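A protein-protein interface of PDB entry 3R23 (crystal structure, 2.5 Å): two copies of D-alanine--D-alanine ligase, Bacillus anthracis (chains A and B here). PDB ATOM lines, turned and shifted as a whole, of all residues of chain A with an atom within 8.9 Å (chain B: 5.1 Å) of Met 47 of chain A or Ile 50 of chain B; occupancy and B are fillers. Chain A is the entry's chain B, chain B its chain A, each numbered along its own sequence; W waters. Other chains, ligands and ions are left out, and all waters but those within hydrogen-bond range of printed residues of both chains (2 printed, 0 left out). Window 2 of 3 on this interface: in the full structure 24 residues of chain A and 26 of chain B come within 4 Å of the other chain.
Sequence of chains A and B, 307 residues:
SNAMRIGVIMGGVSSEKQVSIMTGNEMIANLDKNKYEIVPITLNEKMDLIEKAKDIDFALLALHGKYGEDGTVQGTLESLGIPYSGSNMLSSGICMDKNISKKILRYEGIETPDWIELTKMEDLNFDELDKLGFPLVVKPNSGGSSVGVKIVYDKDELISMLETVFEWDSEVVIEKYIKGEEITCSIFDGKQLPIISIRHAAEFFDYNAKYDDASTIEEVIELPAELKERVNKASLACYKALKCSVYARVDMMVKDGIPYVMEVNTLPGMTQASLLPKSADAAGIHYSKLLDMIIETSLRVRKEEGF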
ATOM      1  N   LEU A  43     -22.656  32.134   8.774  1.00  0.00           N
ATOM      2  CA  LEU A  43     -21.468  31.311   9.011  1.00  0.00           C
ATOM      3  C   LEU A  43     -20.725  31.714  10.287  1.00  0.00           C
ATOM      4  O   LEU A  43     -20.187  32.819  10.378  1.00  0.00           O
ATOM      5  CB  LEU A  43     -20.524  31.377   7.811  1.00  0.00           C
ATOM      6  CG  LEU A  43     -21.116  30.791   6.532  1.00  0.00           C
ATOM      7  CD1 LEU A  43     -20.164  30.951   5.356  1.00  0.00           C
ATOM      8  CD2 LEU A  43     -21.410  29.329   6.758  1.00  0.00           C
ATOM      9  N   ASN A  44     -20.684  30.800  11.258  1.00  0.00           N
ATOM     10  CA  ASN A  44     -19.902  31.005  12.474  1.00  0.00           C
ATOM     11  C   ASN A  44     -18.423  31.000  12.095  1.00  0.00           C
ATOM     12  O   ASN A  44     -17.693  31.975  12.315  1.00  0.00           O
ATOM     13  CB  ASN A  44     -20.231  29.895  13.478  1.00  0.00           C
ATOM     14  CG  ASN A  44     -19.325  29.906  14.698  1.00  0.00           C
ATOM     15  OD1 ASN A  44     -19.268  30.896  15.437  1.00  0.00           O
ATOM     16  ND2 ASN A  44     -18.630  28.790  14.933  1.00  0.00           N
ATOM     17  N   GLU A  45     -18.021  29.896  11.470  1.00  0.00           N
ATOM     18  CA  GLU A  45     -16.736  29.763  10.785  1.00  0.00           C
ATOM     19  C   GLU A  45     -17.031  29.551   9.294  1.00  0.00           C
ATOM     20  O   GLU A  45     -18.082  29.006   8.923  1.00  0.00           O
ATOM     21  CB  GLU A  45     -15.957  28.547  11.309  1.00  0.00           C
ATOM     22  CG  GLU A  45     -15.536  28.596  12.780  1.00  0.00           C
ATOM     23  CD  GLU A  45     -15.112  27.221  13.325  1.00  0.00           C
ATOM     24  OE1 GLU A  45     -14.878  26.280  12.522  1.00  0.00           O
ATOM     25  OE2 GLU A  45     -15.020  27.084  14.566  1.00  0.00           O
ATOM     26  N   LYS A  46     -16.097  29.942   8.439  1.00  0.00           N
ATOM     27  CA  LYS A  46     -16.255  29.702   7.010  1.00  0.00           C
ATOM     28  C   LYS A  46     -16.642  28.247   6.665  1.00  0.00           C
ATOM     29  O   LYS A  46     -17.638  28.017   6.003  1.00  0.00           O
ATOM     30  CB  LYS A  46     -14.986  30.117   6.256  1.00  0.00           C
ATOM     31  CG  LYS A  46     -15.196  30.407   4.770  1.00  0.00           C
ATOM     32  CD  LYS A  46     -13.866  30.618   4.021  1.00  0.00           C
ATOM     33  CE  LYS A  46     -13.203  31.979   4.324  1.00  0.00           C
ATOM     34  NZ  LYS A  46     -12.509  32.561   3.112  1.00  0.00           N
ATOM     35  N   MET A  47     -15.888  27.259   7.124  1.00  0.00           N
ATOM     36  CA  MET A  47     -16.137  25.880   6.671  1.00  0.00           C
ATOM     37  C   MET A  47     -17.415  25.216   7.237  1.00  0.00           C
ATOM     38  O   MET A  47     -17.764  24.102   6.853  1.00  0.00           O
ATOM     39  CB  MET A  47     -14.893  24.999   6.838  1.00  0.00           C
ATOM     40  CG  MET A  47     -13.618  25.594   6.237  1.00  0.00           C
ATOM     41  SD  MET A  47     -13.858  26.377   4.459  1.00  0.00           S
ATOM     42  CE  MET A  47     -14.261  24.836   3.457  1.00  0.00           C
ATOM     43  N   ASP A  48     -18.102  25.909   8.142  1.00  0.00           N
ATOM     44  CA  ASP A  48     -19.418  25.490   8.600  1.00  0.00           C
ATOM     45  C   ASP A  48     -20.370  25.508   7.395  1.00  0.00           C
ATOM     46  O   ASP A  48     -21.473  24.978   7.444  1.00  0.00           O
ATOM     47  CB  ASP A  48     -19.895  26.397   9.753  1.00  0.00           C
ATOM     48  CG  ASP A  48     -18.981  26.300  11.015  1.00  0.00           C
ATOM     49  OD1 ASP A  48     -18.405  25.205  11.248  1.00  0.00           O
ATOM     50  OD2 ASP A  48     -18.836  27.299  11.773  1.00  0.00           O
ATOM     51  N   LEU A  49     -19.906  26.089   6.293  1.00  0.00           N
ATOM     52  CA  LEU A  49     -20.679  26.218   5.055  1.00  0.00           C
ATOM     53  C   LEU A  49     -21.060  24.892   4.420  1.00  0.00           C
ATOM     54  O   LEU A  49     -22.070  24.784   3.743  1.00  0.00           O
ATOM     55  CB  LEU A  49     -19.888  27.046   4.035  1.00  0.00           C
ATOM     56  CG  LEU A  49     -20.385  27.135   2.591  1.00  0.00           C
ATOM     57  CD1 LEU A  49     -21.843  27.533   2.514  1.00  0.00           C
ATOM     58  CD2 LEU A  49     -19.535  28.117   1.834  1.00  0.00           C
ATOM     59  N   ILE A  50     -20.234  23.884   4.619  1.00  0.00           N
ATOM     60  CA  ILE A  50     -20.468  22.593   4.007  1.00  0.00           C
ATOM     61  C   ILE A  50     -21.658  21.912   4.651  1.00  0.00           C
ATOM     62  O   ILE A  50     -22.501  21.339   3.968  1.00  0.00           O
ATOM     63  CB  ILE A  50     -19.243  21.720   4.194  1.00  0.00           C
ATOM     64  CG1 ILE A  50     -18.171  22.112   3.192  1.00  0.00           C
ATOM     65  CG2 ILE A  50     -19.593  20.235   4.112  1.00  0.00           C
ATOM     66  CD1 ILE A  50     -16.819  21.598   3.637  1.00  0.00           C
ATOM     67  N   GLU A  51     -21.711  21.963   5.974  1.00  0.00           N
ATOM     68  CA  GLU A  51     -22.816  21.386   6.712  1.00  0.00           C
ATOM     69  C   GLU A  51     -24.116  22.083   6.302  1.00  0.00           C
ATOM     70  O   GLU A  51     -25.055  21.440   5.835  1.00  0.00           O
ATOM     71  CB  GLU A  51     -22.565  21.599   8.197  1.00  0.00           C
ATOM     72  CG  GLU A  51     -23.040  20.511   9.114  1.00  0.00           C
ATOM     73  CD  GLU A  51     -22.765  20.875  10.571  1.00  0.00           C
ATOM     74  OE1 GLU A  51     -22.151  20.052  11.295  1.00  0.00           O
ATOM     75  OE2 GLU A  51     -23.154  22.001  10.981  1.00  0.00           O
ATOM     76  N   LYS A  52     -24.147  23.406   6.461  1.00  0.00           N
ATOM     77  CA  LYS A  52     -25.337  24.195   6.182  1.00  0.00           C
ATOM     78  C   LYS A  52     -25.798  24.044   4.743  1.00  0.00           C
ATOM     79  O   LYS A  52     -26.982  23.847   4.477  1.00  0.00           O
ATOM     80  CB  LYS A  52     -25.094  25.665   6.513  1.00  0.00           C
ATOM     81  CG  LYS A  52     -24.577  25.896   7.932  1.00  0.00           C
ATOM     82  CD  LYS A  52     -25.323  27.031   8.641  1.00  0.00           C
ATOM     83  CE  LYS A  52     -24.946  27.138  10.124  1.00  0.00           C
ATOM     84  NZ  LYS A  52     -23.474  27.326  10.291  1.00  0.00           N
ATOM     85  N   ALA A  53     -24.863  24.119   3.808  1.00  0.00           N
ATOM     86  CA  ALA A  53     -25.214  24.105   2.387  1.00  0.00           C
ATOM     87  C   ALA A  53     -25.795  22.775   1.957  1.00  0.00           C
ATOM     88  O   ALA A  53     -26.246  22.633   0.816  1.00  0.00           O
ATOM     89  CB  ALA A  53     -24.020  24.462   1.529  1.00  0.00           C
ATOM     90  N   TYR A  67     -13.212  37.952   2.736  1.00  0.00           N
ATOM     91  CA  TYR A  67     -13.864  36.701   3.042  1.00  0.00           C
ATOM     92  C   TYR A  67     -14.665  36.163   1.861  1.00  0.00           C
ATOM     93  O   TYR A  67     -14.724  34.957   1.639  1.00  0.00           O
ATOM     94  CB  TYR A  67     -14.755  36.930   4.234  1.00  0.00           C
ATOM     95  CG  TYR A  67     -15.365  35.705   4.831  1.00  0.00           C
ATOM     96  CD1 TYR A  67     -16.599  35.249   4.388  1.00  0.00           C
ATOM     97  CD2 TYR A  67     -14.746  35.040   5.874  1.00  0.00           C
ATOM     98  CE1 TYR A  67     -17.189  34.157   4.945  1.00  0.00           C
ATOM     99  CE2 TYR A  67     -15.332  33.942   6.451  1.00  0.00           C
ATOM    100  CZ  TYR A  67     -16.558  33.503   5.975  1.00  0.00           C
ATOM    101  OH  TYR A  67     -17.173  32.407   6.520  1.00  0.00           O
ATOM    102  N   ASP A  70     -11.648  36.149  -1.652  1.00  0.00           N
ATOM    103  CA  ASP A  70     -10.392  35.450  -1.832  1.00  0.00           C
ATOM    104  C   ASP A  70     -10.557  34.210  -2.750  1.00  0.00           C
ATOM    105  O   ASP A  70      -9.601  33.732  -3.363  1.00  0.00           O
ATOM    106  CB  ASP A  70      -9.677  35.182  -0.500  1.00  0.00           C
ATOM    107  CG  ASP A  70     -10.351  34.093   0.404  1.00  0.00           C
ATOM    108  OD1 ASP A  70     -11.337  33.420   0.043  1.00  0.00           O
ATOM    109  OD2 ASP A  70      -9.820  33.907   1.521  1.00  0.00           O
ATOM    110  N   THR A  72     -12.057  31.172  -1.641  1.00  0.00           N
ATOM    111  CA  THR A  72     -12.318  29.938  -0.921  1.00  0.00           C
ATOM    112  C   THR A  72     -13.789  29.512  -0.925  1.00  0.00           C
ATOM    113  O   THR A  72     -14.124  28.384  -1.304  1.00  0.00           O
ATOM    114  CB  THR A  72     -11.783  29.966   0.522  1.00  0.00           C
ATOM    115  OG1 THR A  72     -10.386  30.208   0.498  1.00  0.00           O
ATOM    116  CG2 THR A  72     -12.041  28.656   1.213  1.00  0.00           C
ATOM    117  N   VAL A  73     -14.672  30.403  -0.501  1.00  0.00           N
ATOM    118  CA  VAL A  73     -16.103  30.092  -0.508  1.00  0.00           C
ATOM    119  C   VAL A  73     -16.586  29.609  -1.888  1.00  0.00           C
ATOM    120  O   VAL A  73     -17.300  28.634  -1.981  1.00  0.00           O
ATOM    121  CB  VAL A  73     -16.946  31.309  -0.001  1.00  0.00           C
ATOM    122  CG1 VAL A  73     -18.412  31.146  -0.330  1.00  0.00           C
ATOM    123  CG2 VAL A  73     -16.750  31.488   1.498  1.00  0.00           C
ATOM    124  N   GLN A  74     -16.193  30.292  -2.952  1.00  0.00           N
ATOM    125  CA  GLN A  74     -16.551  29.860  -4.297  1.00  0.00           C
ATOM    126  C   GLN A  74     -15.959  28.474  -4.619  1.00  0.00           C
ATOM    127  O   GLN A  74     -16.574  27.675  -5.336  1.00  0.00           O
ATOM    128  CB  GLN A  74     -16.085  30.870  -5.354  1.00  0.00           C
ATOM    129  CG  GLN A  74     -16.733  32.207  -5.276  1.00  0.00           C
ATOM    130  CD  GLN A  74     -16.121  33.086  -4.231  1.00  0.00           C
ATOM    131  OE1 GLN A  74     -15.171  32.691  -3.564  1.00  0.00           O
ATOM    132  NE2 GLN A  74     -16.662  34.292  -4.075  1.00  0.00           N
ATOM    133  N   GLY A  75     -14.748  28.219  -4.125  1.00  0.00           N
ATOM    134  CA  GLY A  75     -14.069  26.962  -4.395  1.00  0.00           C
ATOM    135  C   GLY A  75     -14.774  25.810  -3.696  1.00  0.00           C
ATOM    136  O   GLY A  75     -14.940  24.715  -4.235  1.00  0.00           O
ATOM    137  N   THR A  76     -15.178  26.090  -2.471  1.00  0.00           N
ATOM    138  CA  THR A  76     -15.865  25.170  -1.606  1.00  0.00           C
ATOM    139  C   THR A  76     -17.222  24.832  -2.201  1.00  0.00           C
ATOM    140  O   THR A  76     -17.635  23.683  -2.179  1.00  0.00           O
ATOM    141  CB  THR A  76     -16.079  25.860  -0.269  1.00  0.00           C
ATOM    142  OG1 THR A  76     -14.846  25.898   0.442  1.00  0.00           O
ATOM    143  CG2 THR A  76     -17.130  25.157   0.541  1.00  0.00           C
ATOM    144  N   LEU A  77     -17.918  25.843  -2.729  1.00  0.00           N
ATOM    145  CA  LEU A  77     -19.267  25.642  -3.235  1.00  0.00           C
ATOM    146  C   LEU A  77     -19.232  24.851  -4.543  1.00  0.00           C
ATOM    147  O   LEU A  77     -20.077  23.989  -4.786  1.00  0.00           O
ATOM    148  CB  LEU A  77     -19.969  26.972  -3.408  1.00  0.00           C
ATOM    149  CG  LEU A  77     -20.450  27.639  -2.105  1.00  0.00           C
ATOM    150  CD1 LEU A  77     -20.896  29.094  -2.326  1.00  0.00           C
ATOM    151  CD2 LEU A  77     -21.590  26.867  -1.522  1.00  0.00           C
ATOM    152  N   SER A  79     -17.015  22.604  -5.201  1.00  0.00           N
ATOM    153  CA  SER A  79     -16.679  21.228  -4.809  1.00  0.00           C
ATOM    154  C   SER A  79     -17.858  20.447  -4.253  1.00  0.00           C
ATOM    155  O   SER A  79     -17.906  19.220  -4.390  1.00  0.00           O
ATOM    156  CB  SER A  79     -15.578  21.230  -3.752  1.00  0.00           C
ATOM    157  OG  SER A  79     -14.435  21.837  -4.299  1.00  0.00           O
ATOM    158  N   LEU A  80     -18.777  21.159  -3.603  1.00  0.00           N
ATOM    159  CA  LEU A  80     -20.015  20.563  -3.125  1.00  0.00           C
ATOM    160  C   LEU A  80     -21.017  20.462  -4.276  1.00  0.00           C
ATOM    161  O   LEU A  80     -22.105  19.939  -4.081  1.00  0.00           O
ATOM    162  CB  LEU A  80     -20.641  21.381  -1.979  1.00  0.00           C
ATOM    163  CG  LEU A  80     -19.808  21.572  -0.716  1.00  0.00           C
ATOM    164  CD1 LEU A  80     -20.360  22.671   0.190  1.00  0.00           C
ATOM    165  CD2 LEU A  80     -19.665  20.233   0.033  1.00  0.00           C
ATOM    166  N   MET B  47     -14.488  17.788   0.279  1.00  0.00           N
ATOM    167  CA  MET B  47     -14.780  18.536   1.492  1.00  0.00           C
ATOM    168  C   MET B  47     -14.760  17.667   2.785  1.00  0.00           C
ATOM    169  O   MET B  47     -14.934  18.178   3.888  1.00  0.00           O
ATOM    170  CB  MET B  47     -16.052  19.382   1.323  1.00  0.00           C
ATOM    171  CG  MET B  47     -15.915  20.399   0.211  1.00  0.00           C
ATOM    172  SD  MET B  47     -14.271  21.522   0.231  1.00  0.00           S
ATOM    173  CE  MET B  47     -14.843  22.944   1.382  1.00  0.00           C
ATOM    174  N   ASP B  48     -14.511  16.367   2.641  1.00  0.00           N
ATOM    175  CA  ASP B  48     -14.325  15.485   3.795  1.00  0.00           C
ATOM    176  C   ASP B  48     -13.112  15.944   4.597  1.00  0.00           C
ATOM    177  O   ASP B  48     -12.925  15.563   5.741  1.00  0.00           O
ATOM    178  CB  ASP B  48     -14.132  14.034   3.335  1.00  0.00           C
ATOM    179  CG  ASP B  48     -15.390  13.438   2.744  1.00  0.00           C
ATOM    180  OD1 ASP B  48     -16.486  13.805   3.222  1.00  0.00           O
ATOM    181  OD2 ASP B  48     -15.290  12.606   1.810  1.00  0.00           O
ATOM    182  N   LEU B  49     -12.300  16.766   3.955  1.00  0.00           N
ATOM    183  CA  LEU B  49     -11.055  17.320   4.489  1.00  0.00           C
ATOM    184  C   LEU B  49     -11.236  18.084   5.777  1.00  0.00           C
ATOM    185  O   LEU B  49     -10.390  17.998   6.663  1.00  0.00           O
ATOM    186  CB  LEU B  49     -10.415  18.256   3.453  1.00  0.00           C
ATOM    187  CG  LEU B  49      -9.015  18.830   3.659  1.00  0.00           C
ATOM    188  CD1 LEU B  49      -7.970  17.703   3.830  1.00  0.00           C
ATOM    189  CD2 LEU B  49      -8.622  19.809   2.492  1.00  0.00           C
ATOM    190  N   ILE B  50     -12.330  18.833   5.884  1.00  0.00           N
ATOM    191  CA  ILE B  50     -12.569  19.664   7.061  1.00  0.00           C
ATOM    192  C   ILE B  50     -12.622  18.825   8.325  1.00  0.00           C
ATOM    193  O   ILE B  50     -12.031  19.189   9.349  1.00  0.00           O
ATOM    194  CB  ILE B  50     -13.877  20.522   6.952  1.00  0.00           C
ATOM    195  CG1 ILE B  50     -13.702  21.674   5.963  1.00  0.00           C
ATOM    196  CG2 ILE B  50     -14.281  21.121   8.323  1.00  0.00           C
ATOM    197  CD1 ILE B  50     -13.730  21.258   4.521  1.00  0.00           C
ATOM    198  N   GLU B  51     -13.335  17.706   8.260  1.00  0.00           N
ATOM    199  CA  GLU B  51     -13.424  16.810   9.402  1.00  0.00           C
ATOM    200  C   GLU B  51     -12.157  16.025   9.575  1.00  0.00           C
ATOM    201  O   GLU B  51     -11.612  15.968  10.674  1.00  0.00           O
ATOM    202  CB  GLU B  51     -14.568  15.822   9.220  1.00  0.00           C
ATOM    203  CG  GLU B  51     -15.420  15.647  10.464  1.00  0.00           C
ATOM    204  CD  GLU B  51     -16.896  15.561  10.115  1.00  0.00           C
ATOM    205  OE1 GLU B  51     -17.321  14.514   9.554  1.00  0.00           O
ATOM    206  OE2 GLU B  51     -17.621  16.553  10.381  1.00  0.00           O
ATOM    207  N   LYS B  52     -11.688  15.424   8.484  1.00  0.00           N
ATOM    208  CA  LYS B  52     -10.561  14.500   8.553  1.00  0.00           C
ATOM    209  C   LYS B  52      -9.277  15.210   8.965  1.00  0.00           C
ATOM    210  O   LYS B  52      -8.355  14.567   9.449  1.00  0.00           O
ATOM    211  CB  LYS B  52     -10.367  13.777   7.225  1.00  0.00           C
ATOM    212  CG  LYS B  52     -11.499  12.826   6.933  1.00  0.00           C
ATOM    213  CD  LYS B  52     -11.151  11.849   5.843  1.00  0.00           C
ATOM    214  CE  LYS B  52     -12.138  10.699   5.795  1.00  0.00           C
ATOM    215  NZ  LYS B  52     -11.958   9.843   4.575  1.00  0.00           N
ATOM    216  N   ALA B  53      -9.222  16.532   8.776  1.00  0.00           N
ATOM    217  CA  ALA B  53      -8.028  17.307   9.119  1.00  0.00           C
ATOM    218  C   ALA B  53      -8.098  17.975  10.486  1.00  0.00           C
ATOM    219  O   ALA B  53      -7.172  18.680  10.885  1.00  0.00           O
ATOM    220  CB  ALA B  53      -7.744  18.328   8.057  1.00  0.00           C
ATOM    221  N   LYS B  54      -9.188  17.768  11.209  1.00  0.00           N
ATOM    222  CA  LYS B  54      -9.390  18.514  12.448  1.00  0.00           C
ATOM    223  C   LYS B  54      -8.163  18.484  13.389  1.00  0.00           C
ATOM    224  O   LYS B  54      -7.727  19.535  13.875  1.00  0.00           O
ATOM    225  CB  LYS B  54     -10.693  18.076  13.149  1.00  0.00           C
ATOM    226  CG  LYS B  54     -10.616  17.967  14.679  1.00  0.00           C
ATOM    227  CD  LYS B  54     -11.750  18.729  15.399  1.00  0.00           C
ATOM    228  CE  LYS B  54     -11.822  18.398  16.913  1.00  0.00           C
ATOM    229  NZ  LYS B  54     -10.542  18.593  17.670  1.00  0.00           N
ATOM    230  N   THR B  76      -8.835  26.116   1.687  1.00  0.00           N
ATOM    231  CA  THR B  76      -9.578  25.449   2.739  1.00  0.00           C
ATOM    232  C   THR B  76      -8.681  25.347   3.967  1.00  0.00           C
ATOM    233  O   THR B  76      -9.060  25.759   5.071  1.00  0.00           O
ATOM    234  CB  THR B  76     -10.048  24.054   2.335  1.00  0.00           C
ATOM    235  OG1 THR B  76     -11.038  24.152   1.311  1.00  0.00           O
ATOM    236  CG2 THR B  76     -10.661  23.351   3.509  1.00  0.00           C
ATOM    237  N   SER B  79      -8.048  28.568   5.641  1.00  0.00           N
ATOM    238  CA  SER B  79      -9.162  29.135   6.365  1.00  0.00           C
ATOM    239  C   SER B  79      -9.390  28.399   7.704  1.00  0.00           C
ATOM    240  O   SER B  79     -10.000  28.943   8.610  1.00  0.00           O
ATOM    241  CB  SER B  79     -10.414  29.140   5.494  1.00  0.00           C
ATOM    242  OG  SER B  79     -11.271  28.097   5.900  1.00  0.00           O
ATOM    243  N   LEU B  80      -8.872  27.176   7.812  1.00  0.00           N
ATOM    244  CA  LEU B  80      -8.915  26.389   9.042  1.00  0.00           C
ATOM    245  C   LEU B  80      -7.716  26.656   9.929  1.00  0.00           C
ATOM    246  O   LEU B  80      -7.681  26.155  11.045  1.00  0.00           O
ATOM    247  CB  LEU B  80      -8.922  24.882   8.747  1.00  0.00           C
ATOM    248  CG  LEU B  80     -10.120  24.250   8.056  1.00  0.00           C
ATOM    249  CD1 LEU B  80      -9.824  22.846   7.615  1.00  0.00           C
ATOM    250  CD2 LEU B  80     -11.330  24.271   8.962  1.00  0.00           C
HETATM  251  O   HOH W   1     -13.496  27.828   8.364  1.00  0.00           O
HETATM  252  O   HOH W   2     -16.744  17.647  -1.546  1.00  0.00           O
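The side-chain hydroxyl (OG) of Ser 79 of chain B sits at hydrogen-bond distance from the backbone carbonyl oxygen (O) of Thr 76 of chain B (3.3 Å).
The side-chain hydroxyl of Thr 76 of chain A lies within hydrogen-bond range of the backbone carbonyl oxygen of Thr 72 of chain A (3.1 Å).
Water W1 lies within hydrogen-bond range of N of Met 47 of chain A (2.8 Å), OG of Ser 79 of chain B (3.3 Å) and N of Lys 46 of chain A (3.4 Å).
Water W2 bridges N of Met 47 of chain B (2.9 Å) and O of Ser 79 of chain A (3.5 Å).
Of the 11 printed residues of chain B, 5 touch a printed residue of chain A.
Hydrophobic or aromatic side chains of chain B that line the printed part of chain A: Met 47, Ile 50 and Leu 80.
Along chain B the printed residues that touch a printed residue of chain A span positions 47 to 80.
Of the 21 printed residues of chain A, 4 touch a printed residue of chain B.
Among the printed residues, 9 pairs touch across the chains.
Among the printed residues, no Asp or Glu carboxylate lies within 4 Å of a Lys or Arg side-chain nitrogen of the other chain.
Printed residues of chain B within 4 Å of Met 47 of chain A: Met 47, Ile 50, Thr 76, Ser 79 and Leu 80.
Of the printed residues of chain B, Leu 80 of chain A touches Met 47 (3.8 Å).
Of chain A, only Met 47 (3.6 Å) and Ile 50 (3.2 Å) come within 4 Å of Ile 50 of chain B.
Printed residues of chain A within 4 Å of Ser 79 of chain B: Met 47.
The nearest printed residue of chain B that does not touch Met 47 of chain A is Glu 51 of chain B (7.6 Å).
The nearest residue of chain A that does not touch Ile 50 of chain B is Asp 48 of chain A (6.1 Å).
The nearest printed residue of chain B that does not touch Ile 50 of chain A is Asp 48 of chain B (5.8 Å).
Met 47 of chain A touches its own counterpart, Met 47 of chain B.
Met 47 of chain A touches Ile 50 of chain B, and with the chains exchanged Ile 50 of chain A touches Met 47 of chain B.
Met 47 of chain A touches Thr 76 of chain B, and with the chains exchanged Thr 76 of chain A touches Met 47 of chain B.
Met 47 of chain A touches Leu 80 of chain B, and with the chains exchanged Leu 80 of chain A touches Met 47 of chain B.
CE of Met 47 of chain A touches CE of Met 47 of chain B (2.9 Å).
CB of Met 47 of chain A touches CG1 of Ile 50 of chain B, at 3.6 Å.
Met 47 of chain A touches Thr 76 of chain B (CE to CG2, 3.9 Å).
Met 47 of chain A touches Leu 80 of chain B.
Met 47 of chain B touches Ile 50 of chain A.
Ile 50 of chain A touches Ile 50 of chain B.
Thr 76 of chain A touches Met 47 of chain B.
Leu 80 of chain A touches Met 47 of chain B (CD2 to CG, 3.8 Å).
The side-chain sulfur of Met 47 of chain A is in hydrogen-bond range of the side-chain hydroxyl of Ser 79 of chain B, at 3.4 Å.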
